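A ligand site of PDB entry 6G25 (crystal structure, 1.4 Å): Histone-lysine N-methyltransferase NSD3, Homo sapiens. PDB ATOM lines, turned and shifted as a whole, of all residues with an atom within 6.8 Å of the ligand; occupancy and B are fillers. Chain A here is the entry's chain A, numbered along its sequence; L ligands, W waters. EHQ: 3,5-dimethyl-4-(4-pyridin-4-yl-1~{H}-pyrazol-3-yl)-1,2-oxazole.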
ATOM      1  N   SER A  14      -1.825  10.299  18.859  1.00  0.00           N
ATOM      2  CA  SER A  14      -0.426  10.704  19.039  1.00  0.00           C
ATOM      3  C   SER A  14       0.026  11.557  17.878  1.00  0.00           C
ATOM      4  O   SER A  14      -0.283  11.233  16.722  1.00  0.00           O
ATOM      5  CB  SER A  14       0.495   9.485  19.133  1.00  0.00           C
ATOM      6  OG  SER A  14       0.087   8.595  20.168  1.00  0.00           O
ATOM      7  N   LYS A  15       0.790  12.619  18.165  1.00  0.00           N
ATOM      8  CA  LYS A  15       1.337  13.494  17.134  1.00  0.00           C
ATOM      9  C   LYS A  15       2.842  13.241  17.115  1.00  0.00           C
ATOM     10  O   LYS A  15       3.533  13.615  18.074  1.00  0.00           O
ATOM     11  CB  LYS A  15       1.005  14.960  17.465  1.00  0.00           C
ATOM     12  CG  LYS A  15       1.368  15.960  16.380  1.00  0.00           C
ATOM     13  CD  LYS A  15       0.448  15.833  15.156  1.00  0.00           C
ATOM     14  CE  LYS A  15       0.671  16.967  14.181  1.00  0.00           C
ATOM     15  NZ  LYS A  15       1.891  16.728  13.380  1.00  0.00           N
ATOM     16  N   VAL A  16       3.319  12.507  16.101  1.00  0.00           N
ATOM     17  CA  VAL A  16       4.712  12.086  15.998  1.00  0.00           C
ATOM     18  C   VAL A  16       5.305  12.445  14.635  1.00  0.00           C
ATOM     19  O   VAL A  16       4.748  12.069  13.609  1.00  0.00           O
ATOM     20  CB  VAL A  16       4.815  10.556  16.259  1.00  0.00           C
ATOM     21  CG1 VAL A  16       6.244  10.022  16.033  1.00  0.00           C
ATOM     22  CG2 VAL A  16       4.321  10.198  17.656  1.00  0.00           C
ATOM     23  N   GLY A  17       6.465  13.098  14.653  1.00  0.00           N
ATOM     24  CA  GLY A  17       7.177  13.442  13.433  1.00  0.00           C
ATOM     25  C   GLY A  17       6.381  14.318  12.498  1.00  0.00           C
ATOM     26  O   GLY A  17       5.722  15.265  12.946  1.00  0.00           O
ATOM     27  N   THR A  18       6.438  14.012  11.196  1.00  0.00           N
ATOM     28  CA  THR A  18       5.743  14.782  10.172  1.00  0.00           C
ATOM     29  C   THR A  18       4.310  14.314   9.928  1.00  0.00           C
ATOM     30  O   THR A  18       3.637  14.839   9.029  1.00  0.00           O
ATOM     31  CB  THR A  18       6.544  14.722   8.861  1.00  0.00           C
ATOM     32  OG1 THR A  18       6.659  13.355   8.456  1.00  0.00           O
ATOM     33  CG2 THR A  18       7.934  15.328   9.009  1.00  0.00           C
ATOM     34  N   TYR A  19       3.848  13.355  10.707  1.00  0.00           N
ATOM     35  CA  TYR A  19       2.539  12.793  10.514  1.00  0.00           C
ATOM     36  C   TYR A  19       1.447  13.532  11.246  1.00  0.00           C
ATOM     37  O   TYR A  19       1.694  14.130  12.289  1.00  0.00           O
ATOM     38  CB  TYR A  19       2.542  11.323  10.936  1.00  0.00           C
ATOM     39  CG  TYR A  19       3.341  10.460   9.997  1.00  0.00           C
ATOM     40  CD1 TYR A  19       2.733   9.876   8.878  1.00  0.00           C
ATOM     41  CD2 TYR A  19       4.692  10.240  10.202  1.00  0.00           C
ATOM     42  CE1 TYR A  19       3.473   9.090   7.993  1.00  0.00           C
ATOM     43  CE2 TYR A  19       5.449   9.483   9.299  1.00  0.00           C
ATOM     44  CZ  TYR A  19       4.829   8.900   8.206  1.00  0.00           C
ATOM     45  OH  TYR A  19       5.563   8.125   7.349  1.00  0.00           O
ATOM     46  N   PRO A  20       0.200  13.439  10.742  1.00  0.00           N
ATOM     47  CA  PRO A  20      -0.914  14.066  11.457  1.00  0.00           C
ATOM     48  C   PRO A  20      -1.230  13.328  12.752  1.00  0.00           C
ATOM     49  O   PRO A  20      -0.734  12.228  12.967  1.00  0.00           O
ATOM     50  CB  PRO A  20      -2.075  13.960  10.460  1.00  0.00           C
ATOM     51  CG  PRO A  20      -1.771  12.725   9.672  1.00  0.00           C
ATOM     52  CD  PRO A  20      -0.252  12.745   9.527  1.00  0.00           C
ATOM     53  N   TRP A  22      -2.635  10.818  15.036  1.00  0.00           N
ATOM     54  CA  TRP A  22      -2.866   9.456  14.569  1.00  0.00           C
ATOM     55  C   TRP A  22      -3.465   8.591  15.631  1.00  0.00           C
ATOM     56  O   TRP A  22      -3.011   8.648  16.787  1.00  0.00           O
ATOM     57  CB  TRP A  22      -1.498   8.859  14.144  1.00  0.00           C
ATOM     58  CG  TRP A  22      -1.637   7.783  13.123  1.00  0.00           C
ATOM     59  CD1 TRP A  22      -1.976   6.463  13.330  1.00  0.00           C
ATOM     60  CD2 TRP A  22      -1.567   7.952  11.705  1.00  0.00           C
ATOM     61  NE1 TRP A  22      -2.147   5.827  12.130  1.00  0.00           N
ATOM     62  CE2 TRP A  22      -1.917   6.726  11.110  1.00  0.00           C
ATOM     63  CE3 TRP A  22      -1.256   9.052  10.877  1.00  0.00           C
ATOM     64  CZ2 TRP A  22      -1.878   6.521   9.726  1.00  0.00           C
ATOM     65  CZ3 TRP A  22      -1.253   8.865   9.498  1.00  0.00           C
ATOM     66  CH2 TRP A  22      -1.574   7.620   8.933  1.00  0.00           C
ATOM     67  N   CYS A  24      -3.965   5.593  18.103  1.00  0.00           N
ATOM     68  CA  CYS A  24      -3.024   4.655  18.741  1.00  0.00           C
ATOM     69  C   CYS A  24      -3.665   3.944  19.898  1.00  0.00           C
ATOM     70  O   CYS A  24      -4.702   4.336  20.414  1.00  0.00           O
ATOM     71  CB  CYS A  24      -1.790   5.408  19.260  1.00  0.00           C
ATOM     72  SG  CYS A  24      -0.820   6.273  18.001  1.00  0.00           S
ATOM     73  N   PHE A  50       0.727   2.399  16.786  1.00  0.00           N
ATOM     74  CA  PHE A  50      -0.100   3.115  15.810  1.00  0.00           C
ATOM     75  C   PHE A  50      -1.034   2.127  15.162  1.00  0.00           C
ATOM     76  O   PHE A  50      -0.574   1.069  14.699  1.00  0.00           O
ATOM     77  CB  PHE A  50       0.801   3.721  14.699  1.00  0.00           C
ATOM     78  CG  PHE A  50       1.654   4.832  15.259  1.00  0.00           C
ATOM     79  CD1 PHE A  50       2.799   4.544  16.004  1.00  0.00           C
ATOM     80  CD2 PHE A  50       1.286   6.165  15.098  1.00  0.00           C
ATOM     81  CE1 PHE A  50       3.523   5.563  16.631  1.00  0.00           C
ATOM     82  CE2 PHE A  50       2.029   7.188  15.709  1.00  0.00           C
ATOM     83  CZ  PHE A  50       3.135   6.885  16.462  1.00  0.00           C
ATOM     84  N   PHE A  51      -2.318   2.506  15.029  1.00  0.00           N
ATOM     85  CA  PHE A  51      -3.234   1.689  14.233  1.00  0.00           C
ATOM     86  C   PHE A  51      -2.957   2.063  12.790  1.00  0.00           C
ATOM     87  O   PHE A  51      -3.090   3.224  12.378  1.00  0.00           O
ATOM     88  CB  PHE A  51      -4.695   2.030  14.573  1.00  0.00           C
ATOM     89  CG  PHE A  51      -5.186   1.490  15.890  1.00  0.00           C
ATOM     90  CD1 PHE A  51      -5.455   0.129  16.061  1.00  0.00           C
ATOM     91  CD2 PHE A  51      -5.412   2.337  16.957  1.00  0.00           C
ATOM     92  CE1 PHE A  51      -5.897  -0.366  17.288  1.00  0.00           C
ATOM     93  CE2 PHE A  51      -5.886   1.838  18.171  1.00  0.00           C
ATOM     94  CZ  PHE A  51      -6.151   0.500  18.327  1.00  0.00           C
ATOM     95  N   SER A  52      -2.647   1.042  11.992  1.00  0.00           N
ATOM     96  CA  SER A  52      -2.260   1.226  10.606  1.00  0.00           C
ATOM     97  C   SER A  52      -2.175  -0.128   9.919  1.00  0.00           C
ATOM     98  O   SER A  52      -2.044  -1.135  10.589  1.00  0.00           O
ATOM     99  CB  SER A  52      -0.845   1.774  10.607  1.00  0.00           C
ATOM    100  OG  SER A  52      -0.387   2.035   9.301  1.00  0.00           O
ATOM    101  N   ASN A  53      -2.087  -0.126   8.573  1.00  0.00           N
ATOM    102  CA  ASN A  53      -1.799  -1.364   7.856  1.00  0.00           C
ATOM    103  C   ASN A  53      -0.294  -1.644   7.938  1.00  0.00           C
ATOM    104  O   ASN A  53       0.152  -2.714   7.530  1.00  0.00           O
ATOM    105  CB  ASN A  53      -2.253  -1.248   6.382  1.00  0.00           C
ATOM    106  CG  ASN A  53      -1.486  -0.196   5.610  1.00  0.00           C
ATOM    107  OD1 ASN A  53      -1.234   0.915   6.101  1.00  0.00           O
ATOM    108  ND2 ASN A  53      -1.059  -0.546   4.405  1.00  0.00           N
ATOM    109  N   GLN A  54       0.501  -0.673   8.427  1.00  0.00           N
ATOM    110  CA  GLN A  54       1.944  -0.767   8.610  1.00  0.00           C
ATOM    111  C   GLN A  54       2.195  -0.570  10.118  1.00  0.00           C
ATOM    112  O   GLN A  54       2.413   0.556  10.547  1.00  0.00           O
ATOM    113  CB  GLN A  54       2.657   0.320   7.791  1.00  0.00           C
ATOM    114  CG  GLN A  54       4.194   0.364   7.943  1.00  0.00           C
ATOM    115  CD  GLN A  54       4.735   1.755   8.231  1.00  0.00           C
ATOM    116  OE1 GLN A  54       4.132   2.562   8.957  1.00  0.00           O
ATOM    117  NE2 GLN A  54       5.937   2.040   7.767  1.00  0.00           N
ATOM    118  N   PRO A  55       2.141  -1.641  10.937  1.00  0.00           N
ATOM    119  CA  PRO A  55       2.281  -1.460  12.399  1.00  0.00           C
ATOM    120  C   PRO A  55       3.625  -0.885  12.837  1.00  0.00           C
ATOM    121  O   PRO A  55       4.672  -1.248  12.317  1.00  0.00           O
ATOM    122  CB  PRO A  55       2.057  -2.840  12.989  1.00  0.00           C
ATOM    123  CG  PRO A  55       1.825  -3.755  11.895  1.00  0.00           C
ATOM    124  CD  PRO A  55       1.816  -3.041  10.587  1.00  0.00           C
ATOM    125  N   GLU A  56       3.561   0.070  13.766  1.00  0.00           N
ATOM    126  CA  GLU A  56       4.747   0.743  14.308  1.00  0.00           C
ATOM    127  C   GLU A  56       4.441   1.099  15.740  1.00  0.00           C
ATOM    128  O   GLU A  56       3.288   1.126  16.144  1.00  0.00           O
ATOM    129  CB  GLU A  56       5.073   2.053  13.542  1.00  0.00           C
ATOM    130  CG  GLU A  56       5.334   1.920  12.054  1.00  0.00           C
ATOM    131  CD  GLU A  56       6.660   1.311  11.628  1.00  0.00           C
ATOM    132  OE1 GLU A  56       6.908   1.246  10.406  1.00  0.00           O
ATOM    133  OE2 GLU A  56       7.444   0.890  12.514  1.00  0.00           O
ATOM    134  N   ARG A  57       5.497   1.374  16.505  1.00  0.00           N
ATOM    135  CA  ARG A  57       5.410   1.761  17.897  1.00  0.00           C
ATOM    136  C   ARG A  57       6.317   2.953  18.113  1.00  0.00           C
ATOM    137  O   ARG A  57       7.241   3.184  17.305  1.00  0.00           O
ATOM    138  CB  ARG A  57       5.789   0.597  18.844  1.00  0.00           C
ATOM    139  CG  ARG A  57       7.095  -0.076  18.382  1.00  0.00           C
ATOM    140  CD  ARG A  57       7.879  -0.879  19.399  1.00  0.00           C
ATOM    141  NE  ARG A  57       8.450  -0.053  20.465  1.00  0.00           N
ATOM    142  CZ  ARG A  57       9.572   0.633  20.395  1.00  0.00           C
ATOM    143  NH1 ARG A  57       9.988   1.350  21.432  1.00  0.00           N
ATOM    144  NH2 ARG A  57      10.281   0.660  19.262  1.00  0.00           N
ATOM    145  N   ALA A  58       6.050   3.709  19.176  1.00  0.00           N
ATOM    146  CA  ALA A  58       6.882   4.841  19.518  1.00  0.00           C
ATOM    147  C   ALA A  58       6.698   5.260  20.951  1.00  0.00           C
ATOM    148  O   ALA A  58       5.643   5.051  21.535  1.00  0.00           O
ATOM    149  CB  ALA A  58       6.570   6.032  18.614  1.00  0.00           C
ATOM    150  N   GLU A 102      -1.281   8.821   2.597  1.00  0.00           N
ATOM    151  CA  GLU A 102      -1.311   9.013   4.040  1.00  0.00           C
ATOM    152  C   GLU A 102      -2.750   8.977   4.550  1.00  0.00           C
ATOM    153  O   GLU A 102      -3.021   8.275   5.525  1.00  0.00           O
ATOM    154  CB  GLU A 102      -0.631  10.331   4.414  1.00  0.00           C
ATOM    155  CG  GLU A 102      -0.358  10.499   5.894  1.00  0.00           C
ATOM    156  CD  GLU A 102       0.381  11.787   6.195  1.00  0.00           C
ATOM    157  OE1 GLU A 102      -0.275  12.851   6.229  1.00  0.00           O
ATOM    158  OE2 GLU A 102       1.616  11.735   6.349  1.00  0.00           O
ATOM    159  N   GLN A 105      -4.070   5.442   4.659  1.00  0.00           N
ATOM    160  CA  GLN A 105      -3.499   4.746   5.833  1.00  0.00           C
ATOM    161  C   GLN A 105      -4.193   5.222   7.110  1.00  0.00           C
ATOM    162  O   GLN A 105      -4.477   4.406   7.986  1.00  0.00           O
ATOM    163  CB  GLN A 105      -2.001   5.047   5.992  1.00  0.00           C
ATOM    164  CG  GLN A 105      -1.073   4.182   5.153  1.00  0.00           C
ATOM    165  CD  GLN A 105       0.327   4.162   5.736  1.00  0.00           C
ATOM    166  OE1 GLN A 105       0.979   5.197   5.908  1.00  0.00           O
ATOM    167  NE2 GLN A 105       0.812   2.980   6.082  1.00  0.00           N
ATOM    168  N   TRP A 106      -4.451   6.548   7.219  1.00  0.00           N
ATOM    169  CA  TRP A 106      -5.109   7.147   8.381  1.00  0.00           C
ATOM    170  C   TRP A 106      -6.538   6.634   8.495  1.00  0.00           C
ATOM    171  O   TRP A 106      -6.955   6.260   9.588  1.00  0.00           O
ATOM    172  CB  TRP A 106      -5.099   8.668   8.245  1.00  0.00           C
ATOM    173  CG  TRP A 106      -5.589   9.413   9.453  1.00  0.00           C
ATOM    174  CD1 TRP A 106      -4.826   9.827  10.502  1.00  0.00           C
ATOM    175  CD2 TRP A 106      -6.913   9.904   9.688  1.00  0.00           C
ATOM    176  NE1 TRP A 106      -5.595  10.548  11.386  1.00  0.00           N
ATOM    177  CE2 TRP A 106      -6.873  10.639  10.896  1.00  0.00           C
ATOM    178  CE3 TRP A 106      -8.116   9.857   8.954  1.00  0.00           C
ATOM    179  CZ2 TRP A 106      -8.018  11.253  11.429  1.00  0.00           C
ATOM    180  CZ3 TRP A 106      -9.234  10.482   9.482  1.00  0.00           C
ATOM    181  CH2 TRP A 106      -9.185  11.177  10.697  1.00  0.00           C
HETATM  182  C5  EHQ L   1       6.573   5.836  13.279  1.00  0.00           C
HETATM  183  C8  EHQ L   1       6.039   5.629  11.146  1.00  0.00           C
HETATM  184  C10 EHQ L   1       2.646   8.398  12.621  1.00  0.00           C
HETATM  185  N12 EHQ L   1       1.359   4.018  10.144  1.00  0.00           N
HETATM  186  C13 EHQ L   1       6.678   6.240  14.735  1.00  0.00           C
HETATM  187  C15 EHQ L   1       1.168   5.274   9.748  1.00  0.00           C
HETATM  188  C17 EHQ L   1       1.724   6.336  10.431  1.00  0.00           C
HETATM  189  N9  EHQ L   1       3.584   9.165  13.153  1.00  0.00           N
HETATM  190  C18 EHQ L   1       2.761   4.735  11.904  1.00  0.00           C
HETATM  191  C11 EHQ L   1       2.548   6.078  11.532  1.00  0.00           C
HETATM  192  C1  EHQ L   1       4.587   7.275  12.546  1.00  0.00           C
HETATM  193  C14 EHQ L   1       5.387   5.759   9.795  1.00  0.00           C
HETATM  194  C2  EHQ L   1       5.673   6.289  12.342  1.00  0.00           C
HETATM  195  C16 EHQ L   1       2.124   3.729  11.198  1.00  0.00           C
HETATM  196  N7  EHQ L   1       4.793   8.491  13.096  1.00  0.00           N
HETATM  197  C3  EHQ L   1       3.241   7.197  12.200  1.00  0.00           C
HETATM  198  N4  EHQ L   1       7.068   4.888  11.456  1.00  0.00           N
HETATM  199  O6  EHQ L   1       7.369   4.995  12.644  1.00  0.00           O
HETATM  200  O   HOH W   1       1.366  11.166  14.409  1.00  0.00           O
HETATM  201  O   HOH W   2       9.474   3.429  14.111  1.00  0.00           O
HETATM  202  O   HOH W   3       7.600   9.393  12.516  1.00  0.00           O
HETATM  203  O   HOH W   4       9.087   2.745   9.571  1.00  0.00           O
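The side-chain hydroxyl (OG) of Ser 52 sits at hydrogen-bond distance from the side-chain amide oxygen (OD1) of Asn 53, 3.5 Å away.
The backbone carbonyl oxygen of Trp 22 lies within hydrogen-bond range of the backbone NH of Ser 14, 2.9 Å away.
The backbone NH of Phe 50 sits at hydrogen-bond distance from the backbone carbonyl oxygen of Glu 56, 2.9 Å away.
The backbone carbonyl oxygen (O) of Trp 22 is in hydrogen-bond range of the side-chain sulfur (SG) of Cys 24 (3.5 Å).
The side-chain amide nitrogen (NE2) of Gln 105 is in hydrogen-bond range of the side-chain amide oxygen (OD1) of Asn 53 (2.9 Å).
NZ of Lys 15 is in hydrogen-bond range of O of Tyr 19, at 2.8 Å.
NE2 of Gln 54 lies within hydrogen-bond range of OE1 of Glu 56, 2.9 Å away.
The indole nitrogen of Trp 22 lies within hydrogen-bond range of the backbone carbonyl oxygen of Phe 51, at 2.8 Å.
Water W1 lies within hydrogen-bond range of O of Pro 20 (2.8 Å), O of Ser 14 (2.8 Å), N of Val 16 (2.9 Å) and N9 of the ligand (3.2 Å).
Water W4 lies within hydrogen-bond range of OE1 of Glu 56 (2.8 Å) and N4 of the ligand (3.5 Å).
Merely in contact with the ligand: Tyr 19, Trp 22, Phe 50, Glu 56, Ala 58 and Gln 105.
Hydrophobic or aromatic side chains within 4 Å of the ligand: Val 16, Tyr 19, Trp 22, Phe 50 and Ala 58.
Within 4 Å of the ligand: Val 16, Tyr 19, Trp 22, Phe 50, Ser 52, Gln 54, Glu 56, Ala 58 and Gln 105.
Along chain A the residues within 4 Å of the ligand span positions 16 to 105.
OE1 of Gln 54 sits close to N12 of the ligand (3.3 Å).
The side-chain hydroxyl (OG) of Ser 52 lies within hydrogen-bond range of a nitrogen (N12) of the ligand (2.8 Å).
N9 of the ligand lies within hydrogen-bond range of O of Val 16 (3.2 Å).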
